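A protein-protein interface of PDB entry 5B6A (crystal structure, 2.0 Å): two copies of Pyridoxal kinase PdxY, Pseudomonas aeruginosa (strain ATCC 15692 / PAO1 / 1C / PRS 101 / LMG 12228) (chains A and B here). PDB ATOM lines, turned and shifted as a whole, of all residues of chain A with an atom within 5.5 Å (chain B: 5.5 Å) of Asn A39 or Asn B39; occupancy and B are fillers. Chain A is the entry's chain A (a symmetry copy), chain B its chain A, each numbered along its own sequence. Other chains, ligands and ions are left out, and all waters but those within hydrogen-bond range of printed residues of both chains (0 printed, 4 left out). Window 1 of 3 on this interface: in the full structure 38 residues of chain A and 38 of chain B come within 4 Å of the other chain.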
ATOM      1  N   ALA A   9      -0.498 -17.054  13.861  1.00  0.00           N
ATOM      2  CA  ALA A   9      -1.381 -17.612  12.854  1.00  0.00           C
ATOM      3  C   ALA A   9      -1.599 -19.087  13.137  1.00  0.00           C
ATOM      4  O   ALA A   9      -0.664 -19.898  13.051  1.00  0.00           O
ATOM      5  CB  ALA A   9      -0.789 -17.387  11.457  1.00  0.00           C
ATOM      6  N   GLN A  11      -3.436 -22.213  12.065  1.00  0.00           N
ATOM      7  CA  GLN A  11      -4.146 -22.851  10.970  1.00  0.00           C
ATOM      8  C   GLN A  11      -3.376 -24.066  10.462  1.00  0.00           C
ATOM      9  O   GLN A  11      -2.257 -24.337  10.910  1.00  0.00           O
ATOM     10  CB  GLN A  11      -4.277 -21.889   9.776  1.00  0.00           C
ATOM     11  CG  GLN A  11      -4.830 -20.517  10.065  1.00  0.00           C
ATOM     12  CD  GLN A  11      -4.898 -19.697   8.800  1.00  0.00           C
ATOM     13  OE1 GLN A  11      -3.906 -19.073   8.382  1.00  0.00           O
ATOM     14  NE2 GLN A  11      -6.051 -19.727   8.164  1.00  0.00           N
ATOM     15  N   SER A  12      -3.996 -24.787   9.526  1.00  0.00           N
ATOM     16  CA  SER A  12      -3.381 -25.908   8.812  1.00  0.00           C
ATOM     17  C   SER A  12      -2.063 -25.611   8.097  1.00  0.00           C
ATOM     18  O   SER A  12      -1.810 -24.487   7.640  1.00  0.00           O
ATOM     19  CB  SER A  12      -4.381 -26.408   7.795  1.00  0.00           C
ATOM     20  OG  SER A  12      -5.507 -26.865   8.516  1.00  0.00           O
ATOM     21  N   HIS A  13      -1.234 -26.640   7.964  1.00  0.00           N
ATOM     22  CA  HIS A  13      -0.026 -26.548   7.173  1.00  0.00           C
ATOM     23  C   HIS A  13      -0.033 -27.682   6.184  1.00  0.00           C
ATOM     24  O   HIS A  13      -0.439 -28.807   6.522  1.00  0.00           O
ATOM     25  CB  HIS A  13       1.229 -26.627   8.058  1.00  0.00           C
ATOM     26  CG  HIS A  13       2.509 -26.735   7.277  1.00  0.00           C
ATOM     27  ND1 HIS A  13       2.898 -25.795   6.352  1.00  0.00           N
ATOM     28  CD2 HIS A  13       3.463 -27.699   7.255  1.00  0.00           C
ATOM     29  CE1 HIS A  13       4.040 -26.166   5.798  1.00  0.00           C
ATOM     30  NE2 HIS A  13       4.405 -27.317   6.334  1.00  0.00           N
ATOM     31  N   VAL A  15       2.615 -29.508   3.204  1.00  0.00           N
ATOM     32  CA  VAL A  15       4.038 -29.538   2.812  1.00  0.00           C
ATOM     33  C   VAL A  15       4.182 -29.023   1.376  1.00  0.00           C
ATOM     34  O   VAL A  15       4.989 -28.129   1.101  1.00  0.00           O
ATOM     35  CB  VAL A  15       4.686 -30.933   2.984  1.00  0.00           C
ATOM     36  CG1 VAL A  15       6.150 -30.904   2.510  1.00  0.00           C
ATOM     37  CG2 VAL A  15       4.601 -31.400   4.436  1.00  0.00           C
ATOM     38  N   ASN A  21      -2.108 -21.831   6.850  1.00  0.00           N
ATOM     39  CA  ASN A  21      -0.804 -21.159   7.024  1.00  0.00           C
ATOM     40  C   ASN A  21       0.107 -21.200   5.810  1.00  0.00           C
ATOM     41  O   ASN A  21       0.884 -20.261   5.569  1.00  0.00           O
ATOM     42  CB  ASN A  21      -0.035 -21.671   8.266  1.00  0.00           C
ATOM     43  CG  ASN A  21      -0.519 -21.024   9.557  1.00  0.00           C
ATOM     44  OD1 ASN A  21      -1.279 -20.047   9.520  1.00  0.00           O
ATOM     45  ND2 ASN A  21      -0.132 -21.592  10.710  1.00  0.00           N
ATOM     46  N   PRO A  37       3.936 -18.947  13.142  1.00  0.00           N
ATOM     47  CA  PRO A  37       3.037 -19.952  12.571  1.00  0.00           C
ATOM     48  C   PRO A  37       2.850 -21.138  13.532  1.00  0.00           C
ATOM     49  O   PRO A  37       3.811 -21.879  13.805  1.00  0.00           O
ATOM     50  CB  PRO A  37       3.760 -20.395  11.267  1.00  0.00           C
ATOM     51  CG  PRO A  37       5.019 -19.533  11.160  1.00  0.00           C
ATOM     52  CD  PRO A  37       5.307 -19.097  12.593  1.00  0.00           C
ATOM     53  N   LEU A  38       1.625 -21.284  14.036  1.00  0.00           N
ATOM     54  CA  LEU A  38       1.250 -22.441  14.843  1.00  0.00           C
ATOM     55  C   LEU A  38       0.410 -23.356  13.964  1.00  0.00           C
ATOM     56  O   LEU A  38      -0.776 -23.082  13.711  1.00  0.00           O
ATOM     57  CB  LEU A  38       0.464 -22.001  16.099  1.00  0.00           C
ATOM     58  CG  LEU A  38       0.445 -22.960  17.304  1.00  0.00           C
ATOM     59  CD1 LEU A  38      -0.186 -22.213  18.473  1.00  0.00           C
ATOM     60  CD2 LEU A  38      -0.312 -24.265  17.049  1.00  0.00           C
ATOM     61  N   ASN A  39       1.029 -24.442  13.511  1.00  0.00           N
ATOM     62  CA  ASN A  39       0.396 -25.348  12.563  1.00  0.00           C
ATOM     63  C   ASN A  39      -0.474 -26.369  13.292  1.00  0.00           C
ATOM     64  O   ASN A  39       0.011 -27.119  14.145  1.00  0.00           O
ATOM     65  CB  ASN A  39       1.448 -26.019  11.675  1.00  0.00           C
ATOM     66  CG  ASN A  39       2.284 -25.004  10.911  1.00  0.00           C
ATOM     67  OD1 ASN A  39       1.775 -23.966  10.433  1.00  0.00           O
ATOM     68  ND2 ASN A  39       3.570 -25.307  10.753  1.00  0.00           N
ATOM     69  N   THR A  40      -1.767 -26.359  12.976  1.00  0.00           N
ATOM     70  CA  THR A  40      -2.745 -27.223  13.664  1.00  0.00           C
ATOM     71  C   THR A  40      -2.768 -28.628  13.074  1.00  0.00           C
ATOM     72  O   THR A  40      -3.361 -29.536  13.647  1.00  0.00           O
ATOM     73  CB  THR A  40      -4.167 -26.657  13.568  1.00  0.00           C
ATOM     74  OG1 THR A  40      -4.473 -26.439  12.193  1.00  0.00           O
ATOM     75  CG2 THR A  40      -4.261 -25.350  14.295  1.00  0.00           C
ATOM     76  N   VAL A  41      -2.144 -28.779  11.903  1.00  0.00           N
ATOM     77  CA  VAL A  41      -1.993 -30.063  11.239  1.00  0.00           C
ATOM     78  C   VAL A  41      -0.801 -29.926  10.316  1.00  0.00           C
ATOM     79  O   VAL A  41      -0.418 -28.811   9.962  1.00  0.00           O
ATOM     80  CB  VAL A  41      -3.269 -30.444  10.449  1.00  0.00           C
ATOM     81  CG1 VAL A  41      -3.315 -29.812   9.051  1.00  0.00           C
ATOM     82  CG2 VAL A  41      -3.336 -31.942  10.338  1.00  0.00           C
ATOM     83  N   GLN A  42      -0.208 -31.041   9.927  1.00  0.00           N
ATOM     84  CA  GLN A  42       0.715 -31.044   8.809  1.00  0.00           C
ATOM     85  C   GLN A  42       0.314 -32.180   7.855  1.00  0.00           C
ATOM     86  O   GLN A  42       0.464 -33.362   8.185  1.00  0.00           O
ATOM     87  CB  GLN A  42       2.179 -31.203   9.295  1.00  0.00           C
ATOM     88  CG  GLN A  42       3.175 -31.334   8.154  1.00  0.00           C
ATOM     89  CD  GLN A  42       4.622 -31.169   8.591  1.00  0.00           C
ATOM     90  OE1 GLN A  42       5.343 -30.325   8.065  1.00  0.00           O
ATOM     91  NE2 GLN A  42       5.048 -31.973   9.560  1.00  0.00           N
ATOM     92  N   LEU A  57      -2.563 -32.499  14.823  1.00  0.00           N
ATOM     93  CA  LEU A  57      -2.213 -32.086  16.195  1.00  0.00           C
ATOM     94  C   LEU A  57      -3.439 -32.312  17.139  1.00  0.00           C
ATOM     95  O   LEU A  57      -4.550 -31.872  16.814  1.00  0.00           O
ATOM     96  CB  LEU A  57      -1.777 -30.588  16.169  1.00  0.00           C
ATOM     97  CG  LEU A  57      -0.789 -29.883  17.144  1.00  0.00           C
ATOM     98  CD1 LEU A  57       0.662 -30.352  16.971  1.00  0.00           C
ATOM     99  CD2 LEU A  57      -0.833 -28.351  17.072  1.00  0.00           C
ATOM    100  N   LEU A  65       1.828 -25.034  23.179  1.00  0.00           N
ATOM    101  CA  LEU A  65       2.777 -24.215  22.393  1.00  0.00           C
ATOM    102  C   LEU A  65       2.787 -22.741  22.838  1.00  0.00           C
ATOM    103  O   LEU A  65       3.859 -22.152  23.061  1.00  0.00           O
ATOM    104  CB  LEU A  65       2.519 -24.369  20.880  1.00  0.00           C
ATOM    105  CG  LEU A  65       2.955 -25.734  20.285  1.00  0.00           C
ATOM    106  CD1 LEU A  65       2.369 -25.938  18.900  1.00  0.00           C
ATOM    107  CD2 LEU A  65       4.470 -25.920  20.255  1.00  0.00           C
ATOM    108  N   ALA B   9      12.319 -28.754   2.188  1.00  0.00           N
ATOM    109  CA  ALA B   9      13.141 -28.399   3.331  1.00  0.00           C
ATOM    110  C   ALA B   9      12.671 -29.174   4.548  1.00  0.00           C
ATOM    111  O   ALA B   9      11.551 -28.972   5.041  1.00  0.00           O
ATOM    112  CB  ALA B   9      13.081 -26.885   3.568  1.00  0.00           C
ATOM    113  N   GLN B  11      13.328 -29.912   8.198  1.00  0.00           N
ATOM    114  CA  GLN B  11      13.989 -29.436   9.401  1.00  0.00           C
ATOM    115  C   GLN B  11      12.964 -29.055  10.466  1.00  0.00           C
ATOM    116  O   GLN B  11      11.755 -29.080  10.215  1.00  0.00           O
ATOM    117  CB  GLN B  11      14.803 -28.164   9.105  1.00  0.00           C
ATOM    118  CG  GLN B  11      15.757 -28.222   7.939  1.00  0.00           C
ATOM    119  CD  GLN B  11      16.477 -26.907   7.780  1.00  0.00           C
ATOM    120  OE1 GLN B  11      15.964 -25.962   7.152  1.00  0.00           O
ATOM    121  NE2 GLN B  11      17.646 -26.821   8.379  1.00  0.00           N
ATOM    122  N   SER B  12      13.471 -28.706  11.650  1.00  0.00           N
ATOM    123  CA  SER B  12      12.674 -28.179  12.760  1.00  0.00           C
ATOM    124  C   SER B  12      11.823 -26.947  12.455  1.00  0.00           C
ATOM    125  O   SER B  12      12.169 -26.113  11.605  1.00  0.00           O
ATOM    126  CB  SER B  12      13.623 -27.845  13.887  1.00  0.00           C
ATOM    127  OG  SER B  12      14.241 -29.055  14.278  1.00  0.00           O
ATOM    128  N   HIS B  13      10.721 -26.811  13.184  1.00  0.00           N
ATOM    129  CA  HIS B  13       9.906 -25.617  13.117  1.00  0.00           C
ATOM    130  C   HIS B  13       9.724 -25.103  14.520  1.00  0.00           C
ATOM    131  O   HIS B  13       9.543 -25.896  15.460  1.00  0.00           O
ATOM    132  CB  HIS B  13       8.538 -25.911  12.481  1.00  0.00           C
ATOM    133  CG  HIS B  13       7.576 -24.757  12.564  1.00  0.00           C
ATOM    134  ND1 HIS B  13       7.853 -23.517  12.035  1.00  0.00           N
ATOM    135  CD2 HIS B  13       6.362 -24.648  13.156  1.00  0.00           C
ATOM    136  CE1 HIS B  13       6.849 -22.695  12.289  1.00  0.00           C
ATOM    137  NE2 HIS B  13       5.929 -23.361  12.964  1.00  0.00           N
ATOM    138  N   VAL B  15       7.460 -22.016  16.658  1.00  0.00           N
ATOM    139  CA  VAL B  15       6.302 -21.120  16.473  1.00  0.00           C
ATOM    140  C   VAL B  15       6.762 -19.662  16.593  1.00  0.00           C
ATOM    141  O   VAL B  15       6.479 -18.835  15.720  1.00  0.00           O
ATOM    142  CB  VAL B  15       5.133 -21.430  17.437  1.00  0.00           C
ATOM    143  CG1 VAL B  15       3.985 -20.429  17.225  1.00  0.00           C
ATOM    144  CG2 VAL B  15       4.638 -22.863  17.253  1.00  0.00           C
ATOM    145  N   ASN B  21      13.695 -24.748   9.714  1.00  0.00           N
ATOM    146  CA  ASN B  21      12.769 -24.179   8.712  1.00  0.00           C
ATOM    147  C   ASN B  21      12.274 -22.778   9.019  1.00  0.00           C
ATOM    148  O   ASN B  21      12.028 -21.977   8.100  1.00  0.00           O
ATOM    149  CB  ASN B  21      11.561 -25.104   8.429  1.00  0.00           C
ATOM    150  CG  ASN B  21      11.901 -26.222   7.452  1.00  0.00           C
ATOM    151  OD1 ASN B  21      12.967 -26.198   6.822  1.00  0.00           O
ATOM    152  ND2 ASN B  21      11.030 -27.239   7.356  1.00  0.00           N
ATOM    153  N   PRO B  37       7.862 -26.937   2.959  1.00  0.00           N
ATOM    154  CA  PRO B  37       8.405 -27.102   4.310  1.00  0.00           C
ATOM    155  C   PRO B  37       7.844 -28.365   4.982  1.00  0.00           C
ATOM    156  O   PRO B  37       6.633 -28.442   5.255  1.00  0.00           O
ATOM    157  CB  PRO B  37       7.939 -25.816   5.052  1.00  0.00           C
ATOM    158  CG  PRO B  37       7.203 -24.964   4.016  1.00  0.00           C
ATOM    159  CD  PRO B  37       6.744 -25.963   2.958  1.00  0.00           C
ATOM    160  N   LEU B  38       8.728 -29.333   5.222  1.00  0.00           N
ATOM    161  CA  LEU B  38       8.385 -30.529   5.983  1.00  0.00           C
ATOM    162  C   LEU B  38       8.992 -30.375   7.370  1.00  0.00           C
ATOM    163  O   LEU B  38      10.210 -30.544   7.553  1.00  0.00           O
ATOM    164  CB  LEU B  38       8.918 -31.798   5.281  1.00  0.00           C
ATOM    165  CG  LEU B  38       8.234 -33.139   5.609  1.00  0.00           C
ATOM    166  CD1 LEU B  38       8.775 -34.178   4.635  1.00  0.00           C
ATOM    167  CD2 LEU B  38       8.448 -33.610   7.049  1.00  0.00           C
ATOM    168  N   ASN B  39       8.137 -30.063   8.339  1.00  0.00           N
ATOM    169  CA  ASN B  39       8.584 -29.763   9.692  1.00  0.00           C
ATOM    170  C   ASN B  39       8.749 -31.048  10.500  1.00  0.00           C
ATOM    171  O   ASN B  39       7.800 -31.821  10.663  1.00  0.00           O
ATOM    172  CB  ASN B  39       7.629 -28.777  10.369  1.00  0.00           C
ATOM    173  CG  ASN B  39       7.499 -27.478   9.590  1.00  0.00           C
ATOM    174  OD1 ASN B  39       8.486 -26.954   9.026  1.00  0.00           O
ATOM    175  ND2 ASN B  39       6.290 -26.922   9.579  1.00  0.00           N
ATOM    176  N   THR B  40       9.974 -31.286  10.968  1.00  0.00           N
ATOM    177  CA  THR B  40      10.308 -32.529  11.686  1.00  0.00           C
ATOM    178  C   THR B  40       9.926 -32.449  13.159  1.00  0.00           C
ATOM    179  O   THR B  40       9.934 -33.454  13.862  1.00  0.00           O
ATOM    180  CB  THR B  40      11.807 -32.841  11.612  1.00  0.00           C
ATOM    181  OG1 THR B  40      12.527 -31.704  12.084  1.00  0.00           O
ATOM    182  CG2 THR B  40      12.217 -33.116  10.197  1.00  0.00           C
ATOM    183  N   VAL B  41       9.628 -31.231  13.618  1.00  0.00           N
ATOM    184  CA  VAL B  41       9.162 -30.981  14.971  1.00  0.00           C
ATOM    185  C   VAL B  41       8.413 -29.666  14.927  1.00  0.00           C
ATOM    186  O   VAL B  41       8.614 -28.871  14.008  1.00  0.00           O
ATOM    187  CB  VAL B  41      10.340 -30.917  15.974  1.00  0.00           C
ATOM    188  CG1 VAL B  41      11.001 -29.534  16.027  1.00  0.00           C
ATOM    189  CG2 VAL B  41       9.833 -31.296  17.337  1.00  0.00           C
ATOM    190  N   GLN B  42       7.552 -29.428  15.900  1.00  0.00           N
ATOM    191  CA  GLN B  42       7.036 -28.091  16.129  1.00  0.00           C
ATOM    192  C   GLN B  42       7.190 -27.766  17.624  1.00  0.00           C
ATOM    193  O   GLN B  42       6.501 -28.347  18.470  1.00  0.00           O
ATOM    194  CB  GLN B  42       5.557 -27.980  15.676  1.00  0.00           C
ATOM    195  CG  GLN B  42       4.933 -26.635  16.006  1.00  0.00           C
ATOM    196  CD  GLN B  42       3.611 -26.389  15.296  1.00  0.00           C
ATOM    197  OE1 GLN B  42       3.452 -25.393  14.594  1.00  0.00           O
ATOM    198  NE2 GLN B  42       2.660 -27.302  15.471  1.00  0.00           N
ATOM    199  N   LEU B  57       7.745 -35.047  15.724  1.00  0.00           N
ATOM    200  CA  LEU B  57       7.238 -35.974  14.695  1.00  0.00           C
ATOM    201  C   LEU B  57       7.976 -37.348  14.818  1.00  0.00           C
ATOM    202  O   LEU B  57       9.213 -37.374  14.868  1.00  0.00           O
ATOM    203  CB  LEU B  57       7.457 -35.327  13.291  1.00  0.00           C
ATOM    204  CG  LEU B  57       6.611 -35.569  12.007  1.00  0.00           C
ATOM    205  CD1 LEU B  57       5.195 -34.983  12.103  1.00  0.00           C
ATOM    206  CD2 LEU B  57       7.277 -35.064  10.721  1.00  0.00           C
ATOM    207  N   LEU B  65       4.638 -38.306   4.564  1.00  0.00           N
ATOM    208  CA  LEU B  65       4.339 -37.003   3.934  1.00  0.00           C
ATOM    209  C   LEU B  65       4.797 -36.942   2.465  1.00  0.00           C
ATOM    210  O   LEU B  65       4.030 -36.533   1.577  1.00  0.00           O
ATOM    211  CB  LEU B  65       4.905 -35.838   4.773  1.00  0.00           C
ATOM    212  CG  LEU B  65       4.137 -35.561   6.093  1.00  0.00           C
ATOM    213  CD1 LEU B  65       4.938 -34.653   7.010  1.00  0.00           C
ATOM    214  CD2 LEU B  65       2.739 -34.988   5.866  1.00  0.00           C
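The side-chain amide oxygen (OE1) of Gln B42 sits at hydrogen-bond distance from the backbone NH (N) of Asn A39, 2.8 Å away.
O of Pro B37 lies within hydrogen-bond range of NE2 of His A13, at 2.7 Å.
N of Asn B39 lies within hydrogen-bond range of OE1 of Gln A42 (2.8 Å).
The backbone carbonyl oxygen (O) of Pro A37 sits at hydrogen-bond distance from a ring nitrogen (NE2) of His B13, at 2.7 Å.
The side-chain amide nitrogen (ND2) of Asn B39 lies close to the side-chain amide nitrogen (ND2) of Asn A39 (3.4 Å).
O of Ala A9 is in hydrogen-bond range of N of Leu A38, at 2.9 Å.
The backbone NH (N) of His B13 lies within hydrogen-bond range of the backbone carbonyl oxygen (O) of Val B41, at 3.1 Å.
The backbone carbonyl oxygen (O) of Thr A40 lies close to the backbone NH (N) of Leu A57 (3.3 Å).
N of His A13 is in hydrogen-bond range of O of Val A41 (3.1 Å).
N of Leu B38 lies within hydrogen-bond range of O of Ala B9 (2.9 Å).
The backbone carbonyl oxygen (O) of Leu B38 sits at hydrogen-bond distance from the side-chain amide nitrogen (ND2) of Asn B21, at 3.4 Å.
His A13 touches Asn B39.
O of Val B15 touches CD of Pro A37 (3.3 Å).
Pro A37 touches Gln B42 (O to OE1, 3.6 Å).
CA of Leu A38 touches OE1 of Gln B42, at 3.7 Å.
Asn A39 touches His B13.
Gln A42 touches Pro B37 (OE1 to O, 3.6 Å).
Gln A42 touches Leu B38 (OE1 to CA, 3.7 Å).
Gln A42 touches Leu B57 (NE2 to CD1, 3.9 Å).
Leu A57 touches Gln B42 (CD1 to NE2, 3.9 Å).
Leu A65 touches Gln B42.
Of chain A, only His A13, Asn A39 and Gln A42 come within 4 Å of Asn B39.
Of the printed residues of chain B, Pro A37 touches His B13, Val B15 and Gln B42.
Of the printed residues of chain A, Pro B37 touches His A13, Val A15 and Gln A42.
Printed residues of chain A within 4 Å of His B13: Pro A37 and Asn A39.
Printed residues of chain B within 4 Å of His A13: Pro B37 (2.7 Å) and Asn B39 (3.7 Å).
Of the printed residues of chain A, Leu B38 touches Gln A42 (3.7 Å).
The nearest residue of chain B that does not touch Asn A39 is Val B15 (5.4 Å).
The nearest residue of chain A that does not touch Asn B39 is Val A15 (5.4 Å).
The nearest printed residue of chain A that does not touch Pro B37 is Asn A39 (7.0 Å).
Hydrophobic or aromatic side chains of chain A that line the printed part of chain B: His A13, Val A15, Pro A37, Leu A57 and Leu A65.
Of the 14 printed residues of chain B, 8 touch a printed residue of chain A.
Among the printed residues, 17 pairs touch across the chains.
His A13 touches Asn B39, and with the chains exchanged Asn A39 touches His B13.
Val A15 touches Pro B37, and with the chains exchanged Pro A37 touches Val B15.
Leu A38 touches Gln B42, and with the chains exchanged Gln A42 touches Leu B38.
Asn A39 touches its own counterpart, Asn B39.
14 positions are printed for both chains.
Of the 17 pairs that touch across the chains among the printed residues, 17 have their exchanged pair printed and touching as well.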
